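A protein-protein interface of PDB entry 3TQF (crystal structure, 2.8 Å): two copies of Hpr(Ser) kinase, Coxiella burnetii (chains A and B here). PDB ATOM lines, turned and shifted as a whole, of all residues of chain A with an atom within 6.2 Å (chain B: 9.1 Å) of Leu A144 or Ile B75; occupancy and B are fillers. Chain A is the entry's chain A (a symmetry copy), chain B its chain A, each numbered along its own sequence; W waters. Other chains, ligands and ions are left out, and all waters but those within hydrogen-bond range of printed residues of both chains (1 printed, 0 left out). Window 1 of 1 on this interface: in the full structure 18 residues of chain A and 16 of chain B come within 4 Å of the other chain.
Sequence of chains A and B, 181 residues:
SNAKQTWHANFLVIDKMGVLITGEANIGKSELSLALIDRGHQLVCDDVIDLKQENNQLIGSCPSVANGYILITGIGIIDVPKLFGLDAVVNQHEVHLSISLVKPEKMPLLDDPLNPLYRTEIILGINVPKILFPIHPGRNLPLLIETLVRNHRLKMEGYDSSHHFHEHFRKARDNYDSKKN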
ATOM      1  N   PRO A 113     -13.010 -36.591 -15.168  1.00  0.00           N
ATOM      2  CA  PRO A 113     -13.188 -35.155 -14.914  1.00  0.00           C
ATOM      3  C   PRO A 113     -12.951 -34.724 -13.462  1.00  0.00           C
ATOM      4  O   PRO A 113     -12.951 -33.529 -13.179  1.00  0.00           O
ATOM      5  CB  PRO A 113     -14.645 -34.906 -15.311  1.00  0.00           C
ATOM      6  CG  PRO A 113     -15.326 -36.217 -15.111  1.00  0.00           C
ATOM      7  CD  PRO A 113     -14.299 -37.278 -15.387  1.00  0.00           C
ATOM      8  N   LEU A 114     -12.754 -35.684 -12.559  1.00  0.00           N
ATOM      9  CA  LEU A 114     -12.409 -35.392 -11.166  1.00  0.00           C
ATOM     10  C   LEU A 114     -10.911 -35.127 -10.992  1.00  0.00           C
ATOM     11  O   LEU A 114     -10.469 -34.770  -9.900  1.00  0.00           O
ATOM     12  CB  LEU A 114     -12.840 -36.540 -10.248  1.00  0.00           C
ATOM     13  CG  LEU A 114     -14.347 -36.709 -10.023  1.00  0.00           C
ATOM     14  CD1 LEU A 114     -15.066 -37.156 -11.288  1.00  0.00           C
ATOM     15  CD2 LEU A 114     -14.610 -37.699  -8.896  1.00  0.00           C
ATOM     16  N   ASN A 115     -10.136 -35.312 -12.060  1.00  0.00           N
ATOM     17  CA  ASN A 115      -8.701 -35.021 -12.057  1.00  0.00           C
ATOM     18  C   ASN A 115      -8.296 -34.207 -13.284  1.00  0.00           C
ATOM     19  O   ASN A 115      -9.045 -34.142 -14.255  1.00  0.00           O
ATOM     20  CB  ASN A 115      -7.901 -36.326 -12.005  1.00  0.00           C
ATOM     21  CG  ASN A 115      -7.715 -36.837 -10.591  1.00  0.00           C
ATOM     22  OD1 ASN A 115      -8.352 -37.805 -10.180  1.00  0.00           O
ATOM     23  ND2 ASN A 115      -6.843 -36.177  -9.833  1.00  0.00           N
ATOM     24  N   PRO A 116      -7.107 -33.579 -13.246  1.00  0.00           N
ATOM     25  CA  PRO A 116      -6.628 -32.851 -14.422  1.00  0.00           C
ATOM     26  C   PRO A 116      -6.261 -33.794 -15.560  1.00  0.00           C
ATOM     27  O   PRO A 116      -6.064 -34.988 -15.330  1.00  0.00           O
ATOM     28  CB  PRO A 116      -5.367 -32.130 -13.920  1.00  0.00           C
ATOM     29  CG  PRO A 116      -5.277 -32.386 -12.457  1.00  0.00           C
ATOM     30  CD  PRO A 116      -6.129 -33.560 -12.145  1.00  0.00           C
ATOM     31  N   PHE A 133      -4.432 -27.594 -19.661  1.00  0.00           N
ATOM     32  CA  PHE A 133      -5.403 -26.777 -18.940  1.00  0.00           C
ATOM     33  C   PHE A 133      -6.227 -25.900 -19.873  1.00  0.00           C
ATOM     34  O   PHE A 133      -5.667 -25.112 -20.625  1.00  0.00           O
ATOM     35  CB  PHE A 133      -4.714 -25.899 -17.899  1.00  0.00           C
ATOM     36  CG  PHE A 133      -5.671 -25.288 -16.920  1.00  0.00           C
ATOM     37  CD1 PHE A 133      -6.121 -23.993 -17.083  1.00  0.00           C
ATOM     38  CD2 PHE A 133      -6.155 -26.031 -15.859  1.00  0.00           C
ATOM     39  CE1 PHE A 133      -7.013 -23.441 -16.195  1.00  0.00           C
ATOM     40  CE2 PHE A 133      -7.053 -25.485 -14.967  1.00  0.00           C
ATOM     41  CZ  PHE A 133      -7.482 -24.187 -15.135  1.00  0.00           C
ATOM     42  N   PRO A 134      -7.567 -26.023 -19.810  1.00  0.00           N
ATOM     43  CA  PRO A 134      -8.445 -25.217 -20.647  1.00  0.00           C
ATOM     44  C   PRO A 134      -8.489 -23.768 -20.188  1.00  0.00           C
ATOM     45  O   PRO A 134      -8.687 -23.505 -19.005  1.00  0.00           O
ATOM     46  CB  PRO A 134      -9.806 -25.872 -20.452  1.00  0.00           C
ATOM     47  CG  PRO A 134      -9.748 -26.450 -19.105  1.00  0.00           C
ATOM     48  CD  PRO A 134      -8.336 -26.885 -18.894  1.00  0.00           C
ATOM     49  N   ARG A 139     -11.866 -16.150 -15.484  1.00  0.00           N
ATOM     50  CA  ARG A 139     -12.287 -17.000 -14.371  1.00  0.00           C
ATOM     51  C   ARG A 139     -11.194 -17.018 -13.305  1.00  0.00           C
ATOM     52  O   ARG A 139     -11.110 -17.951 -12.500  1.00  0.00           O
ATOM     53  CB  ARG A 139     -12.585 -18.423 -14.848  1.00  0.00           C
ATOM     54  CG  ARG A 139     -13.645 -18.494 -15.922  1.00  0.00           C
ATOM     55  CD  ARG A 139     -14.202 -19.893 -16.072  1.00  0.00           C
ATOM     56  NE  ARG A 139     -15.198 -19.947 -17.138  1.00  0.00           N
ATOM     57  CZ  ARG A 139     -15.848 -21.045 -17.508  1.00  0.00           C
ATOM     58  NH1 ARG A 139     -15.622 -22.205 -16.902  1.00  0.00           N
ATOM     59  NH2 ARG A 139     -16.733 -20.984 -18.493  1.00  0.00           N
ATOM     60  N   ASN A 140     -10.374 -15.968 -13.303  1.00  0.00           N
ATOM     61  CA  ASN A 140      -9.257 -15.827 -12.377  1.00  0.00           C
ATOM     62  C   ASN A 140      -8.225 -16.918 -12.616  1.00  0.00           C
ATOM     63  O   ASN A 140      -7.894 -17.689 -11.719  1.00  0.00           O
ATOM     64  CB  ASN A 140      -9.748 -15.808 -10.920  1.00  0.00           C
ATOM     65  CG  ASN A 140      -8.873 -14.936 -10.009  1.00  0.00           C
ATOM     66  OD1 ASN A 140      -7.634 -14.912 -10.123  1.00  0.00           O
ATOM     67  ND2 ASN A 140      -9.526 -14.212  -9.098  1.00  0.00           N
ATOM     68  N   LEU A 141      -7.705 -16.945 -13.840  1.00  0.00           N
ATOM     69  CA  LEU A 141      -6.685 -17.913 -14.258  1.00  0.00           C
ATOM     70  C   LEU A 141      -5.470 -18.006 -13.321  1.00  0.00           C
ATOM     71  O   LEU A 141      -4.960 -19.099 -13.101  1.00  0.00           O
ATOM     72  CB  LEU A 141      -6.226 -17.606 -15.689  1.00  0.00           C
ATOM     73  CG  LEU A 141      -5.205 -18.545 -16.335  1.00  0.00           C
ATOM     74  CD1 LEU A 141      -5.731 -19.962 -16.420  1.00  0.00           C
ATOM     75  CD2 LEU A 141      -4.831 -18.031 -17.716  1.00  0.00           C
ATOM     76  N   PRO A 142      -4.996 -16.873 -12.772  1.00  0.00           N
ATOM     77  CA  PRO A 142      -3.875 -16.983 -11.835  1.00  0.00           C
ATOM     78  C   PRO A 142      -4.199 -17.863 -10.641  1.00  0.00           C
ATOM     79  O   PRO A 142      -3.383 -18.704 -10.256  1.00  0.00           O
ATOM     80  CB  PRO A 142      -3.649 -15.541 -11.384  1.00  0.00           C
ATOM     81  CG  PRO A 142      -4.154 -14.720 -12.505  1.00  0.00           C
ATOM     82  CD  PRO A 142      -5.332 -15.465 -13.047  1.00  0.00           C
ATOM     83  N   LEU A 143      -5.386 -17.680 -10.070  1.00  0.00           N
ATOM     84  CA  LEU A 143      -5.813 -18.485  -8.931  1.00  0.00           C
ATOM     85  C   LEU A 143      -5.969 -19.942  -9.347  1.00  0.00           C
ATOM     86  O   LEU A 143      -5.656 -20.842  -8.579  1.00  0.00           O
ATOM     87  CB  LEU A 143      -7.128 -17.954  -8.355  1.00  0.00           C
ATOM     88  CG  LEU A 143      -7.720 -18.720  -7.169  1.00  0.00           C
ATOM     89  CD1 LEU A 143      -6.852 -18.573  -5.940  1.00  0.00           C
ATOM     90  CD2 LEU A 143      -9.129 -18.243  -6.891  1.00  0.00           C
ATOM     91  N   LEU A 144      -6.451 -20.168 -10.564  1.00  0.00           N
ATOM     92  CA  LEU A 144      -6.670 -21.521 -11.050  1.00  0.00           C
ATOM     93  C   LEU A 144      -5.356 -22.263 -11.223  1.00  0.00           C
ATOM     94  O   LEU A 144      -5.220 -23.406 -10.794  1.00  0.00           O
ATOM     95  CB  LEU A 144      -7.449 -21.499 -12.369  1.00  0.00           C
ATOM     96  CG  LEU A 144      -8.859 -20.889 -12.306  1.00  0.00           C
ATOM     97  CD1 LEU A 144      -9.588 -21.103 -13.619  1.00  0.00           C
ATOM     98  CD2 LEU A 144      -9.653 -21.459 -11.153  1.00  0.00           C
ATOM     99  N   ILE A 145      -4.386 -21.593 -11.834  1.00  0.00           N
ATOM    100  CA  ILE A 145      -3.059 -22.162 -12.053  1.00  0.00           C
ATOM    101  C   ILE A 145      -2.320 -22.375 -10.735  1.00  0.00           C
ATOM    102  O   ILE A 145      -1.646 -23.382 -10.557  1.00  0.00           O
ATOM    103  CB  ILE A 145      -2.231 -21.265 -12.986  1.00  0.00           C
ATOM    104  CG1 ILE A 145      -2.834 -21.274 -14.394  1.00  0.00           C
ATOM    105  CG2 ILE A 145      -0.767 -21.718 -13.035  1.00  0.00           C
ATOM    106  CD1 ILE A 145      -2.680 -22.588 -15.126  1.00  0.00           C
ATOM    107  N   GLU A 146      -2.451 -21.438  -9.807  1.00  0.00           N
ATOM    108  CA  GLU A 146      -1.870 -21.610  -8.472  1.00  0.00           C
ATOM    109  C   GLU A 146      -2.466 -22.822  -7.772  1.00  0.00           C
ATOM    110  O   GLU A 146      -1.754 -23.590  -7.138  1.00  0.00           O
ATOM    111  CB  GLU A 146      -2.089 -20.358  -7.615  1.00  0.00           C
ATOM    112  CG  GLU A 146      -1.666 -20.517  -6.156  1.00  0.00           C
ATOM    113  CD  GLU A 146      -2.008 -19.309  -5.322  1.00  0.00           C
ATOM    114  OE1 GLU A 146      -1.263 -18.313  -5.369  1.00  0.00           O
ATOM    115  OE2 GLU A 146      -3.030 -19.350  -4.615  1.00  0.00           O
ATOM    116  N   THR A 147      -3.779 -22.979  -7.886  1.00  0.00           N
ATOM    117  CA  THR A 147      -4.486 -24.100  -7.270  1.00  0.00           C
ATOM    118  C   THR A 147      -4.112 -25.424  -7.938  1.00  0.00           C
ATOM    119  O   THR A 147      -3.938 -26.436  -7.260  1.00  0.00           O
ATOM    120  CB  THR A 147      -6.008 -23.893  -7.335  1.00  0.00           C
ATOM    121  OG1 THR A 147      -6.333 -22.615  -6.777  1.00  0.00           O
ATOM    122  CG2 THR A 147      -6.733 -24.972  -6.556  1.00  0.00           C
ATOM    123  N   LEU A 148      -3.984 -25.403  -9.264  1.00  0.00           N
ATOM    124  CA  LEU A 148      -3.556 -26.575 -10.026  1.00  0.00           C
ATOM    125  C   LEU A 148      -2.181 -27.055  -9.586  1.00  0.00           C
ATOM    126  O   LEU A 148      -1.940 -28.261  -9.497  1.00  0.00           O
ATOM    127  CB  LEU A 148      -3.504 -26.245 -11.513  1.00  0.00           C
ATOM    128  CG  LEU A 148      -3.252 -27.405 -12.469  1.00  0.00           C
ATOM    129  CD1 LEU A 148      -4.499 -28.266 -12.613  1.00  0.00           C
ATOM    130  CD2 LEU A 148      -2.812 -26.869 -13.816  1.00  0.00           C
ATOM    131  N   VAL A 149      -1.281 -26.108  -9.324  1.00  0.00           N
ATOM    132  CA  VAL A 149       0.105 -26.423  -8.970  1.00  0.00           C
ATOM    133  C   VAL A 149       0.197 -26.950  -7.549  1.00  0.00           C
ATOM    134  O   VAL A 149       0.935 -27.889  -7.288  1.00  0.00           O
ATOM    135  CB  VAL A 149       1.032 -25.191  -9.132  1.00  0.00           C
ATOM    136  CG1 VAL A 149       2.425 -25.482  -8.597  1.00  0.00           C
ATOM    137  CG2 VAL A 149       1.107 -24.770 -10.595  1.00  0.00           C
ATOM    138  N   ASN A 151      -2.192 -28.468  -5.910  1.00  0.00           N
ATOM    139  CA  ASN A 151      -2.771 -29.809  -5.981  1.00  0.00           C
ATOM    140  C   ASN A 151      -1.772 -30.814  -6.509  1.00  0.00           C
ATOM    141  O   ASN A 151      -1.717 -31.949  -6.036  1.00  0.00           O
ATOM    142  CB  ASN A 151      -4.028 -29.831  -6.869  1.00  0.00           C
ATOM    143  CG  ASN A 151      -5.315 -29.767  -6.070  1.00  0.00           C
ATOM    144  OD1 ASN A 151      -5.335 -29.310  -4.932  1.00  0.00           O
ATOM    145  ND2 ASN A 151      -6.398 -30.236  -6.667  1.00  0.00           N
ATOM    146  N   GLY B  28     -18.519 -20.410 -15.175  1.00  0.00           N
ATOM    147  CA  GLY B  28     -17.523 -20.096 -14.152  1.00  0.00           C
ATOM    148  C   GLY B  28     -18.059 -19.953 -12.735  1.00  0.00           C
ATOM    149  O   GLY B  28     -17.482 -19.218 -11.931  1.00  0.00           O
ATOM    150  N   SER B  30     -18.310 -22.432 -10.308  1.00  0.00           N
ATOM    151  CA  SER B  30     -17.370 -23.093  -9.392  1.00  0.00           C
ATOM    152  C   SER B  30     -16.064 -22.308  -9.270  1.00  0.00           C
ATOM    153  O   SER B  30     -15.447 -22.272  -8.207  1.00  0.00           O
ATOM    154  CB  SER B  30     -17.079 -24.523  -9.853  1.00  0.00           C
ATOM    155  OG  SER B  30     -18.195 -25.372  -9.620  1.00  0.00           O
ATOM    156  N   GLU B  31     -15.658 -21.675 -10.365  1.00  0.00           N
ATOM    157  CA  GLU B  31     -14.503 -20.796 -10.366  1.00  0.00           C
ATOM    158  C   GLU B  31     -14.776 -19.559  -9.516  1.00  0.00           C
ATOM    159  O   GLU B  31     -13.879 -19.042  -8.863  1.00  0.00           O
ATOM    160  CB  GLU B  31     -14.138 -20.399 -11.795  1.00  0.00           C
ATOM    161  CG  GLU B  31     -13.528 -21.531 -12.631  1.00  0.00           C
ATOM    162  CD  GLU B  31     -14.558 -22.373 -13.395  1.00  0.00           C
ATOM    163  OE1 GLU B  31     -15.633 -22.688 -12.845  1.00  0.00           O
ATOM    164  OE2 GLU B  31     -14.276 -22.737 -14.558  1.00  0.00           O
ATOM    165  N   LEU B  32     -16.020 -19.091  -9.520  1.00  0.00           N
ATOM    166  CA  LEU B  32     -16.420 -17.967  -8.676  1.00  0.00           C
ATOM    167  C   LEU B  32     -16.361 -18.329  -7.196  1.00  0.00           C
ATOM    168  O   LEU B  32     -15.906 -17.522  -6.379  1.00  0.00           O
ATOM    169  CB  LEU B  32     -17.824 -17.481  -9.039  1.00  0.00           C
ATOM    170  CG  LEU B  32     -18.414 -16.341  -8.205  1.00  0.00           C
ATOM    171  CD1 LEU B  32     -17.459 -15.163  -8.138  1.00  0.00           C
ATOM    172  CD2 LEU B  32     -19.767 -15.918  -8.774  1.00  0.00           C
ATOM    173  N   SER B  33     -16.821 -19.532  -6.849  1.00  0.00           N
ATOM    174  CA  SER B  33     -16.743 -20.005  -5.465  1.00  0.00           C
ATOM    175  C   SER B  33     -15.299 -19.976  -4.983  1.00  0.00           C
ATOM    176  O   SER B  33     -15.004 -19.380  -3.953  1.00  0.00           O
ATOM    177  CB  SER B  33     -17.312 -21.420  -5.324  1.00  0.00           C
ATOM    178  OG  SER B  33     -18.726 -21.426  -5.444  1.00  0.00           O
ATOM    179  N   LEU B  34     -14.406 -20.592  -5.750  1.00  0.00           N
ATOM    180  CA  LEU B  34     -12.987 -20.620  -5.415  1.00  0.00           C
ATOM    181  C   LEU B  34     -12.449 -19.212  -5.169  1.00  0.00           C
ATOM    182  O   LEU B  34     -11.823 -18.954  -4.144  1.00  0.00           O
ATOM    183  CB  LEU B  34     -12.177 -21.301  -6.529  1.00  0.00           C
ATOM    184  CG  LEU B  34     -10.714 -21.655  -6.202  1.00  0.00           C
ATOM    185  CD1 LEU B  34     -10.634 -22.651  -5.061  1.00  0.00           C
ATOM    186  CD2 LEU B  34      -9.988 -22.198  -7.429  1.00  0.00           C
ATOM    187  N   ALA B  35     -12.705 -18.301  -6.103  1.00  0.00           N
ATOM    188  CA  ALA B  35     -12.237 -16.918  -5.983  1.00  0.00           C
ATOM    189  C   ALA B  35     -12.779 -16.244  -4.721  1.00  0.00           C
ATOM    190  O   ALA B  35     -12.043 -15.547  -4.027  1.00  0.00           O
ATOM    191  CB  ALA B  35     -12.614 -16.121  -7.214  1.00  0.00           C
ATOM    192  N   ASP B  38     -10.938 -17.444  -1.784  1.00  0.00           N
ATOM    193  CA  ASP B  38      -9.621 -16.802  -1.789  1.00  0.00           C
ATOM    194  C   ASP B  38      -9.675 -15.385  -1.228  1.00  0.00           C
ATOM    195  O   ASP B  38      -8.682 -14.887  -0.712  1.00  0.00           O
ATOM    196  CB  ASP B  38      -9.054 -16.786  -3.216  1.00  0.00           C
ATOM    197  CG  ASP B  38      -7.636 -16.244  -3.286  1.00  0.00           C
ATOM    198  OD1 ASP B  38      -6.742 -16.803  -2.616  1.00  0.00           O
ATOM    199  OD2 ASP B  38      -7.417 -15.260  -4.024  1.00  0.00           O
ATOM    200  N   ILE B  70     -14.893 -29.040  -4.069  1.00  0.00           N
ATOM    201  CA  ILE B  70     -15.339 -28.247  -5.215  1.00  0.00           C
ATOM    202  C   ILE B  70     -14.754 -28.875  -6.468  1.00  0.00           C
ATOM    203  O   ILE B  70     -13.608 -29.303  -6.458  1.00  0.00           O
ATOM    204  CB  ILE B  70     -14.814 -26.791  -5.127  1.00  0.00           C
ATOM    205  CG1 ILE B  70     -15.662 -25.966  -4.168  1.00  0.00           C
ATOM    206  CG2 ILE B  70     -14.811 -26.107  -6.492  1.00  0.00           C
ATOM    207  CD1 ILE B  70     -15.223 -24.500  -4.091  1.00  0.00           C
ATOM    208  N   LEU B  71     -15.536 -28.930  -7.539  1.00  0.00           N
ATOM    209  CA  LEU B  71     -15.042 -29.401  -8.827  1.00  0.00           C
ATOM    210  C   LEU B  71     -14.866 -28.213  -9.770  1.00  0.00           C
ATOM    211  O   LEU B  71     -15.784 -27.407  -9.945  1.00  0.00           O
ATOM    212  CB  LEU B  71     -16.010 -30.418  -9.432  1.00  0.00           C
ATOM    213  CG  LEU B  71     -15.665 -30.955 -10.827  1.00  0.00           C
ATOM    214  CD1 LEU B  71     -14.381 -31.777 -10.798  1.00  0.00           C
ATOM    215  CD2 LEU B  71     -16.814 -31.784 -11.381  1.00  0.00           C
ATOM    216  N   ILE B  72     -13.680 -28.105 -10.365  1.00  0.00           N
ATOM    217  CA  ILE B  72     -13.390 -27.086 -11.366  1.00  0.00           C
ATOM    218  C   ILE B  72     -12.715 -27.767 -12.545  1.00  0.00           C
ATOM    219  O   ILE B  72     -11.662 -28.382 -12.387  1.00  0.00           O
ATOM    220  CB  ILE B  72     -12.465 -25.989 -10.810  1.00  0.00           C
ATOM    221  CG1 ILE B  72     -13.180 -25.196  -9.710  1.00  0.00           C
ATOM    222  CG2 ILE B  72     -12.017 -25.051 -11.919  1.00  0.00           C
ATOM    223  CD1 ILE B  72     -12.352 -24.062  -9.142  1.00  0.00           C
ATOM    224  N   THR B  73     -13.327 -27.671 -13.721  1.00  0.00           N
ATOM    225  CA  THR B  73     -12.816 -28.372 -14.890  1.00  0.00           C
ATOM    226  C   THR B  73     -11.435 -27.840 -15.241  1.00  0.00           C
ATOM    227  O   THR B  73     -11.223 -26.636 -15.313  1.00  0.00           O
ATOM    228  CB  THR B  73     -13.765 -28.247 -16.098  1.00  0.00           C
ATOM    229  OG1 THR B  73     -14.013 -26.864 -16.374  1.00  0.00           O
ATOM    230  CG2 THR B  73     -15.098 -28.959 -15.813  1.00  0.00           C
ATOM    231  N   GLY B  74     -10.494 -28.754 -15.434  1.00  0.00           N
ATOM    232  CA  GLY B  74      -9.092 -28.407 -15.620  1.00  0.00           C
ATOM    233  C   GLY B  74      -8.287 -28.788 -14.397  1.00  0.00           C
ATOM    234  O   GLY B  74      -7.201 -29.340 -14.514  1.00  0.00           O
ATOM    235  N   ILE B  75      -8.835 -28.486 -13.222  1.00  0.00           N
ATOM    236  CA  ILE B  75      -8.206 -28.803 -11.947  1.00  0.00           C
ATOM    237  C   ILE B  75      -8.666 -30.163 -11.447  1.00  0.00           C
ATOM    238  O   ILE B  75      -7.846 -31.006 -11.070  1.00  0.00           O
ATOM    239  CB  ILE B  75      -8.560 -27.759 -10.876  1.00  0.00           C
ATOM    240  CG1 ILE B  75      -8.150 -26.357 -11.334  1.00  0.00           C
ATOM    241  CG2 ILE B  75      -7.884 -28.103  -9.559  1.00  0.00           C
ATOM    242  CD1 ILE B  75      -8.616 -25.245 -10.402  1.00  0.00           C
ATOM    243  N   GLY B  76      -9.982 -30.362 -11.447  1.00  0.00           N
ATOM    244  CA  GLY B  76     -10.605 -31.555 -10.873  1.00  0.00           C
ATOM    245  C   GLY B  76     -11.181 -31.240  -9.506  1.00  0.00           C
ATOM    246  O   GLY B  76     -11.710 -30.158  -9.287  1.00  0.00           O
ATOM    247  N   ILE B  77     -11.068 -32.180  -8.579  1.00  0.00           N
ATOM    248  CA  ILE B  77     -11.556 -31.981  -7.220  1.00  0.00           C
ATOM    249  C   ILE B  77     -10.593 -31.107  -6.416  1.00  0.00           C
ATOM    250  O   ILE B  77      -9.376 -31.194  -6.582  1.00  0.00           O
ATOM    251  CB  ILE B  77     -11.763 -33.336  -6.507  1.00  0.00           C
ATOM    252  CG1 ILE B  77     -12.943 -34.080  -7.136  1.00  0.00           C
ATOM    253  CG2 ILE B  77     -12.016 -33.144  -5.017  1.00  0.00           C
ATOM    254  CD1 ILE B  77     -14.281 -33.378  -6.939  1.00  0.00           C
ATOM    255  N   ILE B  78     -11.153 -30.263  -5.554  1.00  0.00           N
ATOM    256  CA  ILE B  78     -10.377 -29.386  -4.695  1.00  0.00           C
ATOM    257  C   ILE B  78     -10.821 -29.581  -3.249  1.00  0.00           C
ATOM    258  O   ILE B  78     -11.935 -29.201  -2.886  1.00  0.00           O
ATOM    259  CB  ILE B  78     -10.584 -27.896  -5.070  1.00  0.00           C
ATOM    260  CG1 ILE B  78     -10.193 -27.636  -6.526  1.00  0.00           C
ATOM    261  CG2 ILE B  78      -9.775 -26.988  -4.145  1.00  0.00           C
ATOM    262  CD1 ILE B  78     -10.535 -26.239  -7.002  1.00  0.00           C
ATOM    263  N   ASP B  79      -9.953 -30.180  -2.437  1.00  0.00           N
ATOM    264  CA  ASP B  79     -10.169 -30.278  -0.993  1.00  0.00           C
ATOM    265  C   ASP B  79      -9.948 -28.891  -0.400  1.00  0.00           C
ATOM    266  O   ASP B  79      -8.831 -28.542  -0.031  1.00  0.00           O
ATOM    267  CB  ASP B  79      -9.202 -31.302  -0.380  1.00  0.00           C
ATOM    268  CG  ASP B  79      -9.503 -31.611   1.086  1.00  0.00           C
ATOM    269  OD1 ASP B  79     -10.246 -30.852   1.737  1.00  0.00           O
ATOM    270  OD2 ASP B  79      -8.979 -32.630   1.591  1.00  0.00           O
ATOM    271  N   LEU B  83      -6.519 -26.851   1.410  1.00  0.00           N
ATOM    272  CA  LEU B  83      -5.837 -25.763   0.705  1.00  0.00           C
ATOM    273  C   LEU B  83      -6.078 -24.375   1.293  1.00  0.00           C
ATOM    274  O   LEU B  83      -5.241 -23.493   1.132  1.00  0.00           O
ATOM    275  CB  LEU B  83      -6.234 -25.746  -0.780  1.00  0.00           C
ATOM    276  CG  LEU B  83      -5.745 -26.880  -1.690  1.00  0.00           C
ATOM    277  CD1 LEU B  83      -5.955 -26.500  -3.143  1.00  0.00           C
ATOM    278  CD2 LEU B  83      -4.288 -27.220  -1.452  1.00  0.00           C
ATOM    279  N   PHE B  84      -7.218 -24.169   1.948  1.00  0.00           N
ATOM    280  CA  PHE B  84      -7.595 -22.833   2.435  1.00  0.00           C
ATOM    281  C   PHE B  84      -7.898 -22.749   3.939  1.00  0.00           C
ATOM    282  O   PHE B  84      -8.256 -21.680   4.436  1.00  0.00           O
ATOM    283  CB  PHE B  84      -8.781 -22.314   1.618  1.00  0.00           C
ATOM    284  CG  PHE B  84      -8.475 -22.164   0.151  1.00  0.00           C
ATOM    285  CD1 PHE B  84      -7.914 -20.991  -0.338  1.00  0.00           C
ATOM    286  CD2 PHE B  84      -8.732 -23.200  -0.736  1.00  0.00           C
ATOM    287  CE1 PHE B  84      -7.618 -20.852  -1.689  1.00  0.00           C
ATOM    288  CE2 PHE B  84      -8.438 -23.068  -2.090  1.00  0.00           C
ATOM    289  CZ  PHE B  84      -7.882 -21.893  -2.566  1.00  0.00           C
HETATM  290  O   HOH W   1      -6.881 -30.568  -3.325  1.00  0.00           O
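The backbone nitrogen of Pro A116 lies close to the backbone carbonyl oxygen of Ile B75 (3.4 Å). The backbone carbonyl oxygen (O) of Leu A114 lies within hydrogen-bond range of the backbone NH (N) of Ile B77, 3.0 Å away. The backbone carbonyl oxygen of Ile B77 sits at hydrogen-bond distance from the side-chain amide nitrogen of Asn A151 (3.1 Å). The side-chain carboxylate (OE2) of Glu B31 lies within salt-bridge range of the guanidinium group (NH1) of Arg A139 (2.8 Å).
O of Leu A143 sits at hydrogen-bond distance from OG1 of Thr A147 (2.6 Å). OG of Ser B30 lies close to O of Leu B71.
Among the printed residues, merely in contact across the chains: Pro A113 with Leu B71 (3.3 Å), Pro A113 with Gly B76 (3.8 Å), Leu A114 with Gly B76 (3.4 Å), Asn A115 with Ile B75 (3.9 Å), Asn A115 with Gly B76 (3.97 Å), Pro A116 with Gly B74 (3.4 Å), Phe A133 with Gly B74 (3.6 Å), Phe A133 with Ile B75 (3.9 Å), Pro A134 with Gly B74 (3.7 Å), Arg A139 with Gly B28 (3.6 Å), Leu A143 with Leu B34 (3.8 Å), Leu A143 with Ala B35 (3.5 Å), Leu A143 with Asp B38 (3.6 Å), Leu A144 with Leu B34 (3.8 Å), Leu A144 with Ile B75 (3.9 Å), Thr A147 with Leu B34 (3.7 Å), Thr A147 with Leu B83 (3.8 Å), Leu A148 with Gly B74 (3.5 Å), Leu A148 with Ile B75 (3.8 Å), Asn A151 with Ile B75 (3.9 Å) and Asn A151 with Leu B83 (3.4 Å).
Printed residues of chain B within 4 Å of Pro A116: Gly B74 and Ile B75. Printed residues of chain B within 4 Å of Arg A139: Gly B28 (3.6 Å) and Glu B31 (2.8 Å). Leu A143 touches three residues of chain B. Leu A144 touches just these residues of chain B: Leu B34 (3.8 Å) and Ile B75 (3.9 Å). Of the printed residues of chain B, Leu A148 touches Gly B74 (3.5 Å) and Ile B75 (3.8 Å). Of the printed residues of chain B, Asn A151 touches Ile B75 (3.9 Å), Ile B77 (3.1 Å) and Leu B83 (3.4 Å). Of the printed residues of chain A, Gly B74 touches Pro A116 (3.4 Å), Phe A133 (3.6 Å), Pro A134 (3.7 Å) and Leu A148 (3.5 Å). Of chain A, only Asn A115 (3.9 Å), Pro A116 (3.2 Å), Phe A133 (3.9 Å), Leu A144 (3.9 Å), Leu A148 (3.8 Å) and Asn A151 (3.9 Å) come within 4 Å of Ile B75. The nearest residue of chain B that does not touch Leu A144 is Glu B31 (4.1 Å).
Of the 18 printed residues of chain A, 12 touch a printed residue of chain B. Printed residues of chain A that touch a printed residue of chain B: Pro A113, Leu A114, Asn A115, Pro A116, Phe A133, Pro A134, Arg A139, Leu A143, Leu A144, Thr A147, Leu A148 and Asn A151. Hydrophobic or aromatic side chains of chain A that line the printed part of chain B: Leu A114, Pro A116, Phe A133, Pro A134, Leu A143, Leu A144 and Leu A148. Among the printed residues, 25 pairs touch across the chains. Among the printed residues, Asp or Glu carboxylates within 4 Å of a Lys or Arg side-chain nitrogen of the other chain: Arg A139 with Glu B31 (2.8 Å).
No position is printed for both chains. Of the 25 pairs that touch across the chains among the printed residues, none has its exchanged pair printed and touching as well.
Water W1 lies within hydrogen-bond range of the side-chain amide oxygen of Asn A151 and the backbone NH of Asp B79.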
